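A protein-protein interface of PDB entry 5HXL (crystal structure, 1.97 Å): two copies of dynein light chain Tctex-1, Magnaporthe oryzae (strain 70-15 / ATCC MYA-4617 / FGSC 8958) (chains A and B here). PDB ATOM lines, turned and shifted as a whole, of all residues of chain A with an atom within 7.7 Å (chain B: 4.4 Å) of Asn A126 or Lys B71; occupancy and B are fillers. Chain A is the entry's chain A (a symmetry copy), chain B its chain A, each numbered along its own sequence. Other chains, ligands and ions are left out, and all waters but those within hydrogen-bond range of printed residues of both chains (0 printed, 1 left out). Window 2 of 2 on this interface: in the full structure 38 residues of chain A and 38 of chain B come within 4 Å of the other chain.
The side-chain carboxylate of Asp A130 is in salt-bridge range of the side-chain amino group of Lys B71 (2.7 Å).
O of Ala A155 is in hydrogen-bond range of NZ of Lys B71 (3.4 Å).
The backbone NH of Phe A124 lies within hydrogen-bond range of the backbone carbonyl oxygen of Phe B72, at 2.7 Å.
Asn A126 touches just one residue of chain B: Lys B71 (3.7 Å).
Of the printed residues of chain B, Ile A154 touches Lys B71 (3.6 Å) and Ile B154 (3.7 Å).
Of the printed residues of chain B, Ala A155 touches Lys B71 (3.4 Å).
Of the printed residues of chain A, Phe B70 touches Phe A124.
Of chain A, only Phe A124, Asn A126, Asp A130, Ile A154 and Ala A155 come within 4 Å of Lys B71.
Trp B153 touches none of the printed residues of chain A.
Of the printed residues of chain A, Ile B154 touches Ile A154 (3.7 Å).
The nearest printed residue of chain B that does not touch Asn A126 is Phe B72 (7.4 Å).
The nearest printed residue of chain A that does not touch Phe B72 is Trp A125 (4.5 Å).
Among the printed residues, pairs that only touch across the chains: Phe A124 with Lys B71 (3.2 Å), Ala A123 with Phe B72 (3.2 Å), Ile A154 with Lys B71 (3.6 Å), Asn A126 with Lys B71 (3.7 Å), Phe A124 with Phe B70 (3.7 Å) and Ile A154 with Ile B154 (3.7 Å).
Printed residues of chain B that touch a printed residue of chain A: Phe B70, Lys B71, Phe B72 and Ile B154.
Hydrophobic or aromatic side chains of chain B within 4 Å of the printed part of chain A: Ile B154.
Of the 17 printed residues of chain A, 6 touch a printed residue of chain B.
Ile B154 touches its own counterpart, Ile A154.
Of the 9 pairs that touch across the chains among the printed residues, 1 has its exchanged pair printed and touching as well.
O of Ile B154 lies within hydrogen-bond range of N of Lys B71, at 2.8 Å.
The backbone NH (N) of Gly A8 sits at hydrogen-bond distance from the backbone carbonyl oxygen (O) of Asp A130 (2.8 Å).
The backbone NH (N) of Lys A128 is in hydrogen-bond range of the side-chain amide oxygen (OD1) of Asn A126 (3.0 Å).
The side-chain carboxylate (OD2) of Asp A130 sits at hydrogen-bond distance from the backbone NH (N) of Asn A126 (2.9 Å).
The side-chain hydroxyl (OG1) of Thr A129 sits at hydrogen-bond distance from the side-chain carboxylate (OD1) of Asp A130, 2.8 Å away.
The side-chain carboxylate (OD1) of Asp A130 lies within hydrogen-bond range of the backbone NH (N) of Ala A155 (2.7 Å).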
ATOM      1  N   ALA A   6     -29.216  -9.015 -28.950  1.00  0.00           N
ATOM      2  CA  ALA A   6     -28.464  -9.861 -28.014  1.00  0.00           C
ATOM      3  C   ALA A   6     -27.958  -9.048 -26.829  1.00  0.00           C
ATOM      4  O   ALA A   6     -27.750  -7.835 -26.954  1.00  0.00           O
ATOM      5  CB  ALA A   6     -27.297 -10.537 -28.729  1.00  0.00           C
ATOM      6  N   GLN A   7     -27.734  -9.692 -25.682  1.00  0.00           N
ATOM      7  CA  GLN A   7     -27.405  -8.902 -24.489  1.00  0.00           C
ATOM      8  C   GLN A   7     -26.615  -9.579 -23.363  1.00  0.00           C
ATOM      9  O   GLN A   7     -26.560 -10.801 -23.262  1.00  0.00           O
ATOM     10  CB  GLN A   7     -28.703  -8.342 -23.897  1.00  0.00           C
ATOM     11  CG  GLN A   7     -29.514  -9.314 -23.061  1.00  0.00           C
ATOM     12  CD  GLN A   7     -30.711  -8.617 -22.399  1.00  0.00           C
ATOM     13  OE1 GLN A   7     -31.334  -7.741 -22.992  1.00  0.00           O
ATOM     14  NE2 GLN A   7     -30.997  -8.974 -21.152  1.00  0.00           N
ATOM     15  N   GLY A   8     -26.018  -8.743 -22.512  1.00  0.00           N
ATOM     16  CA  GLY A   8     -25.240  -9.191 -21.369  1.00  0.00           C
ATOM     17  C   GLY A   8     -26.061  -9.457 -20.117  1.00  0.00           C
ATOM     18  O   GLY A   8     -27.251  -9.123 -20.055  1.00  0.00           O
ATOM     19  N   PRO A   9     -25.425 -10.067 -19.104  1.00  0.00           N
ATOM     20  CA  PRO A   9     -26.067 -10.358 -17.821  1.00  0.00           C
ATOM     21  C   PRO A   9     -26.402  -9.096 -17.039  1.00  0.00           C
ATOM     22  O   PRO A   9     -25.662  -8.116 -17.100  1.00  0.00           O
ATOM     23  CB  PRO A   9     -25.008 -11.180 -17.082  1.00  0.00           C
ATOM     24  CG  PRO A   9     -23.727 -10.725 -17.661  1.00  0.00           C
ATOM     25  CD  PRO A   9     -24.018 -10.510 -19.116  1.00  0.00           C
ATOM     26  N   ALA A 123     -31.428  -2.596 -30.347  1.00  0.00           N
ATOM     27  CA  ALA A 123     -30.359  -1.773 -29.796  1.00  0.00           C
ATOM     28  C   ALA A 123     -29.075  -1.818 -30.608  1.00  0.00           C
ATOM     29  O   ALA A 123     -28.819  -2.755 -31.350  1.00  0.00           O
ATOM     30  CB  ALA A 123     -30.065  -2.193 -28.362  1.00  0.00           C
ATOM     31  N   PHE A 124     -28.263  -0.791 -30.403  1.00  0.00           N
ATOM     32  CA  PHE A 124     -26.926  -0.693 -30.945  1.00  0.00           C
ATOM     33  C   PHE A 124     -26.075  -0.481 -29.716  1.00  0.00           C
ATOM     34  O   PHE A 124     -25.918   0.652 -29.256  1.00  0.00           O
ATOM     35  CB  PHE A 124     -26.833   0.466 -31.941  1.00  0.00           C
ATOM     36  CG  PHE A 124     -25.458   0.662 -32.551  1.00  0.00           C
ATOM     37  CD1 PHE A 124     -24.987  -0.210 -33.511  1.00  0.00           C
ATOM     38  CD2 PHE A 124     -24.683   1.762 -32.213  1.00  0.00           C
ATOM     39  CE1 PHE A 124     -23.743  -0.025 -34.084  1.00  0.00           C
ATOM     40  CE2 PHE A 124     -23.440   1.955 -32.789  1.00  0.00           C
ATOM     41  CZ  PHE A 124     -22.969   1.060 -33.722  1.00  0.00           C
ATOM     42  N   TRP A 125     -25.610  -1.573 -29.115  1.00  0.00           N
ATOM     43  CA  TRP A 125     -24.893  -1.451 -27.840  1.00  0.00           C
ATOM     44  C   TRP A 125     -23.848  -2.545 -27.696  1.00  0.00           C
ATOM     45  O   TRP A 125     -23.485  -3.205 -28.672  1.00  0.00           O
ATOM     46  CB  TRP A 125     -25.839  -1.503 -26.635  1.00  0.00           C
ATOM     47  CG  TRP A 125     -26.729  -2.707 -26.566  1.00  0.00           C
ATOM     48  CD1 TRP A 125     -26.447  -3.973 -27.015  1.00  0.00           C
ATOM     49  CD2 TRP A 125     -27.930  -2.832 -25.789  1.00  0.00           C
ATOM     50  NE1 TRP A 125     -27.464  -4.839 -26.688  1.00  0.00           N
ATOM     51  CE2 TRP A 125     -28.374  -4.172 -25.915  1.00  0.00           C
ATOM     52  CE3 TRP A 125     -28.690  -1.937 -25.036  1.00  0.00           C
ATOM     53  CZ2 TRP A 125     -29.555  -4.628 -25.334  1.00  0.00           C
ATOM     54  CZ3 TRP A 125     -29.884  -2.399 -24.464  1.00  0.00           C
ATOM     55  CH2 TRP A 125     -30.288  -3.729 -24.610  1.00  0.00           C
ATOM     56  N   ASN A 126     -23.375  -2.755 -26.471  1.00  0.00           N
ATOM     57  CA  ASN A 126     -22.368  -3.785 -26.225  1.00  0.00           C
ATOM     58  C   ASN A 126     -23.081  -5.060 -25.792  1.00  0.00           C
ATOM     59  O   ASN A 126     -23.562  -5.154 -24.671  1.00  0.00           O
ATOM     60  CB  ASN A 126     -21.346  -3.324 -25.163  1.00  0.00           C
ATOM     61  CG  ASN A 126     -20.155  -4.274 -25.032  1.00  0.00           C
ATOM     62  OD1 ASN A 126     -20.293  -5.479 -25.227  1.00  0.00           O
ATOM     63  ND2 ASN A 126     -18.982  -3.729 -24.690  1.00  0.00           N
ATOM     64  N   ASP A 127     -23.123  -6.051 -26.682  1.00  0.00           N
ATOM     65  CA  ASP A 127     -23.899  -7.268 -26.439  1.00  0.00           C
ATOM     66  C   ASP A 127     -23.339  -8.113 -25.295  1.00  0.00           C
ATOM     67  O   ASP A 127     -24.020  -9.002 -24.781  1.00  0.00           O
ATOM     68  CB  ASP A 127     -23.976  -8.115 -27.711  1.00  0.00           C
ATOM     69  CG  ASP A 127     -24.498  -7.331 -28.908  1.00  0.00           C
ATOM     70  OD1 ASP A 127     -25.394  -6.474 -28.728  1.00  0.00           O
ATOM     71  OD2 ASP A 127     -24.003  -7.565 -30.031  1.00  0.00           O
ATOM     72  N   LYS A 128     -22.096  -7.853 -24.895  1.00  0.00           N
ATOM     73  CA  LYS A 128     -21.499  -8.603 -23.785  1.00  0.00           C
ATOM     74  C   LYS A 128     -21.905  -8.070 -22.411  1.00  0.00           C
ATOM     75  O   LYS A 128     -21.818  -8.791 -21.402  1.00  0.00           O
ATOM     76  CB  LYS A 128     -19.966  -8.584 -23.878  1.00  0.00           C
ATOM     77  CG  LYS A 128     -19.376  -9.293 -25.098  1.00  0.00           C
ATOM     78  CD  LYS A 128     -17.841  -9.193 -25.052  1.00  0.00           C
ATOM     79  CE  LYS A 128     -17.208  -9.888 -26.249  1.00  0.00           C
ATOM     80  NZ  LYS A 128     -17.648  -9.295 -27.542  1.00  0.00           N
ATOM     81  N   THR A 129     -22.306  -6.802 -22.353  1.00  0.00           N
ATOM     82  CA  THR A 129     -22.499  -6.144 -21.058  1.00  0.00           C
ATOM     83  C   THR A 129     -23.837  -5.428 -20.879  1.00  0.00           C
ATOM     84  O   THR A 129     -24.293  -5.260 -19.754  1.00  0.00           O
ATOM     85  CB  THR A 129     -21.393  -5.092 -20.784  1.00  0.00           C
ATOM     86  OG1 THR A 129     -21.455  -4.057 -21.779  1.00  0.00           O
ATOM     87  CG2 THR A 129     -20.005  -5.722 -20.769  1.00  0.00           C
ATOM     88  N   ASP A 130     -24.458  -4.998 -21.972  1.00  0.00           N
ATOM     89  CA  ASP A 130     -25.661  -4.160 -21.875  1.00  0.00           C
ATOM     90  C   ASP A 130     -26.924  -4.993 -22.039  1.00  0.00           C
ATOM     91  O   ASP A 130     -26.887  -6.066 -22.617  1.00  0.00           O
ATOM     92  CB  ASP A 130     -25.610  -3.048 -22.921  1.00  0.00           C
ATOM     93  CG  ASP A 130     -24.310  -2.253 -22.865  1.00  0.00           C
ATOM     94  OD1 ASP A 130     -23.635  -2.253 -21.803  1.00  0.00           O
ATOM     95  OD2 ASP A 130     -23.955  -1.637 -23.889  1.00  0.00           O
ATOM     96  N   GLY A 131     -28.051  -4.515 -21.527  1.00  0.00           N
ATOM     97  CA  GLY A 131     -29.265  -5.295 -21.671  1.00  0.00           C
ATOM     98  C   GLY A 131     -30.495  -4.621 -21.140  1.00  0.00           C
ATOM     99  O   GLY A 131     -30.462  -3.475 -20.678  1.00  0.00           O
ATOM    100  N   TRP A 153     -29.820  -1.404 -18.791  1.00  0.00           N
ATOM    101  CA  TRP A 153     -28.512  -1.113 -18.208  1.00  0.00           C
ATOM    102  C   TRP A 153     -27.444  -1.043 -19.290  1.00  0.00           C
ATOM    103  O   TRP A 153     -27.455  -1.811 -20.248  1.00  0.00           O
ATOM    104  CB  TRP A 153     -28.114  -2.154 -17.159  1.00  0.00           C
ATOM    105  CG  TRP A 153     -28.021  -3.559 -17.671  1.00  0.00           C
ATOM    106  CD1 TRP A 153     -26.920  -4.182 -18.204  1.00  0.00           C
ATOM    107  CD2 TRP A 153     -29.071  -4.517 -17.681  1.00  0.00           C
ATOM    108  NE1 TRP A 153     -27.233  -5.479 -18.540  1.00  0.00           N
ATOM    109  CE2 TRP A 153     -28.545  -5.708 -18.230  1.00  0.00           C
ATOM    110  CE3 TRP A 153     -30.411  -4.485 -17.275  1.00  0.00           C
ATOM    111  CZ2 TRP A 153     -29.318  -6.858 -18.385  1.00  0.00           C
ATOM    112  CZ3 TRP A 153     -31.176  -5.640 -17.432  1.00  0.00           C
ATOM    113  CH2 TRP A 153     -30.628  -6.798 -17.980  1.00  0.00           C
ATOM    114  N   ILE A 154     -26.534  -0.094 -19.127  1.00  0.00           N
ATOM    115  CA  ILE A 154     -25.510   0.184 -20.114  1.00  0.00           C
ATOM    116  C   ILE A 154     -24.178   0.295 -19.399  1.00  0.00           C
ATOM    117  O   ILE A 154     -24.012   1.155 -18.548  1.00  0.00           O
ATOM    118  CB  ILE A 154     -25.798   1.499 -20.891  1.00  0.00           C
ATOM    119  CG1 ILE A 154     -27.171   1.456 -21.580  1.00  0.00           C
ATOM    120  CG2 ILE A 154     -24.660   1.804 -21.855  1.00  0.00           C
ATOM    121  CD1 ILE A 154     -27.234   0.555 -22.824  1.00  0.00           C
ATOM    122  N   ALA A 155     -23.237  -0.583 -19.733  1.00  0.00           N
ATOM    123  CA  ALA A 155     -21.939  -0.603 -19.073  1.00  0.00           C
ATOM    124  C   ALA A 155     -21.141   0.643 -19.397  1.00  0.00           C
ATOM    125  O   ALA A 155     -21.159   1.126 -20.531  1.00  0.00           O
ATOM    126  CB  ALA A 155     -21.150  -1.845 -19.465  1.00  0.00           C
ATOM    127  N   VAL A 156     -20.446   1.130 -18.370  1.00  0.00           N
ATOM    128  CA  VAL A 156     -19.489   2.230 -18.438  1.00  0.00           C
ATOM    129  C   VAL A 156     -20.166   3.532 -18.835  1.00  0.00           C
ATOM    130  O   VAL A 156     -20.620   4.280 -17.967  1.00  0.00           O
ATOM    131  CB  VAL A 156     -18.328   1.912 -19.408  1.00  0.00           C
ATOM    132  CG1 VAL A 156     -17.598   3.185 -19.814  1.00  0.00           C
ATOM    133  CG2 VAL A 156     -17.373   0.905 -18.770  1.00  0.00           C
ATOM    134  N   PHE B  70     -21.866   6.738 -29.615  1.00  0.00           N
ATOM    135  CA  PHE B  70     -23.142   6.582 -28.908  1.00  0.00           C
ATOM    136  C   PHE B  70     -23.697   5.175 -29.034  1.00  0.00           C
ATOM    137  O   PHE B  70     -23.640   4.574 -30.102  1.00  0.00           O
ATOM    138  CB  PHE B  70     -24.188   7.588 -29.433  1.00  0.00           C
ATOM    139  CG  PHE B  70     -23.896   9.015 -29.068  1.00  0.00           C
ATOM    140  CD1 PHE B  70     -24.331   9.534 -27.865  1.00  0.00           C
ATOM    141  CD2 PHE B  70     -23.168   9.835 -29.927  1.00  0.00           C
ATOM    142  CE1 PHE B  70     -24.049  10.845 -27.519  1.00  0.00           C
ATOM    143  CE2 PHE B  70     -22.884  11.136 -29.591  1.00  0.00           C
ATOM    144  CZ  PHE B  70     -23.324  11.649 -28.390  1.00  0.00           C
ATOM    145  N   LYS B  71     -24.217   4.649 -27.929  1.00  0.00           N
ATOM    146  CA  LYS B  71     -25.059   3.462 -27.967  1.00  0.00           C
ATOM    147  C   LYS B  71     -26.504   3.925 -28.142  1.00  0.00           C
ATOM    148  O   LYS B  71     -26.858   5.035 -27.720  1.00  0.00           O
ATOM    149  CB  LYS B  71     -24.903   2.623 -26.686  1.00  0.00           C
ATOM    150  CG  LYS B  71     -23.453   2.122 -26.462  1.00  0.00           C
ATOM    151  CD  LYS B  71     -23.335   1.346 -25.158  1.00  0.00           C
ATOM    152  CE  LYS B  71     -21.948   0.681 -25.022  1.00  0.00           C
ATOM    153  NZ  LYS B  71     -21.816   0.000 -23.705  1.00  0.00           N
ATOM    154  N   PHE B  72     -27.331   3.083 -28.755  1.00  0.00           N
ATOM    155  CA  PHE B  72     -28.752   3.386 -28.907  1.00  0.00           C
ATOM    156  C   PHE B  72     -29.613   2.238 -28.486  1.00  0.00           C
ATOM    157  O   PHE B  72     -29.267   1.081 -28.711  1.00  0.00           O
ATOM    158  CB  PHE B  72     -29.107   3.720 -30.354  1.00  0.00           C
ATOM    159  CG  PHE B  72     -28.390   4.901 -30.883  1.00  0.00           C
ATOM    160  CD1 PHE B  72     -28.761   6.172 -30.496  1.00  0.00           C
ATOM    161  CD2 PHE B  72     -27.337   4.748 -31.770  1.00  0.00           C
ATOM    162  CE1 PHE B  72     -28.089   7.276 -30.974  1.00  0.00           C
ATOM    163  CE2 PHE B  72     -26.670   5.846 -32.256  1.00  0.00           C
ATOM    164  CZ  PHE B  72     -27.050   7.114 -31.854  1.00  0.00           C
ATOM    165  N   ILE B 152     -33.352   6.067 -26.978  1.00  0.00           N
ATOM    166  CA  ILE B 152     -32.410   6.466 -25.941  1.00  0.00           C
ATOM    167  C   ILE B 152     -31.016   6.502 -26.573  1.00  0.00           C
ATOM    168  O   ILE B 152     -30.666   5.589 -27.317  1.00  0.00           O
ATOM    169  CB  ILE B 152     -32.405   5.472 -24.747  1.00  0.00           C
ATOM    170  CG1 ILE B 152     -33.779   5.408 -24.062  1.00  0.00           C
ATOM    171  CG2 ILE B 152     -31.300   5.816 -23.740  1.00  0.00           C
ATOM    172  CD1 ILE B 152     -33.902   6.293 -22.855  1.00  0.00           C
ATOM    173  N   TRP B 153     -30.237   7.551 -26.311  1.00  0.00           N
ATOM    174  CA  TRP B 153     -28.828   7.548 -26.700  1.00  0.00           C
ATOM    175  C   TRP B 153     -27.932   7.687 -25.478  1.00  0.00           C
ATOM    176  O   TRP B 153     -28.238   8.422 -24.542  1.00  0.00           O
ATOM    177  CB  TRP B 153     -28.514   8.666 -27.697  1.00  0.00           C
ATOM    178  CG  TRP B 153     -28.790  10.051 -27.199  1.00  0.00           C
ATOM    179  CD1 TRP B 153     -27.931  10.883 -26.527  1.00  0.00           C
ATOM    180  CD2 TRP B 153     -30.009  10.767 -27.351  1.00  0.00           C
ATOM    181  NE1 TRP B 153     -28.553  12.081 -26.257  1.00  0.00           N
ATOM    182  CE2 TRP B 153     -29.827  12.034 -26.752  1.00  0.00           C
ATOM    183  CE3 TRP B 153     -31.242  10.461 -27.941  1.00  0.00           C
ATOM    184  CZ2 TRP B 153     -30.837  12.993 -26.724  1.00  0.00           C
ATOM    185  CZ3 TRP B 153     -32.245  11.428 -27.910  1.00  0.00           C
ATOM    186  CH2 TRP B 153     -32.035  12.667 -27.307  1.00  0.00           C
ATOM    187  N   ILE B 154     -26.829   6.953 -25.497  1.00  0.00           N
ATOM    188  CA  ILE B 154     -25.919   6.881 -24.372  1.00  0.00           C
ATOM    189  C   ILE B 154     -24.506   7.062 -24.891  1.00  0.00           C
ATOM    190  O   ILE B 154     -24.046   6.269 -25.696  1.00  0.00           O
ATOM    191  CB  ILE B 154     -26.032   5.524 -23.623  1.00  0.00           C
ATOM    192  CG1 ILE B 154     -27.465   5.267 -23.135  1.00  0.00           C
ATOM    193  CG2 ILE B 154     -25.002   5.449 -22.505  1.00  0.00           C
ATOM    194  CD1 ILE B 154     -27.891   6.116 -21.926  1.00  0.00           C
ATOM    195  N   VAL B 156     -20.575   7.044 -25.372  1.00  0.00           N
ATOM    196  CA  VAL B 156     -19.429   6.168 -25.153  1.00  0.00           C
ATOM    197  C   VAL B 156     -19.867   4.747 -24.836  1.00  0.00           C
ATOM    198  O   VAL B 156     -20.027   3.934 -25.748  1.00  0.00           O
ATOM    199  CB  VAL B 156     -18.508   6.708 -24.034  1.00  0.00           C
ATOM    200  CG1 VAL B 156     -17.592   5.610 -23.511  1.00  0.00           C
ATOM    201  CG2 VAL B 156     -17.706   7.902 -24.547  1.00  0.00           C
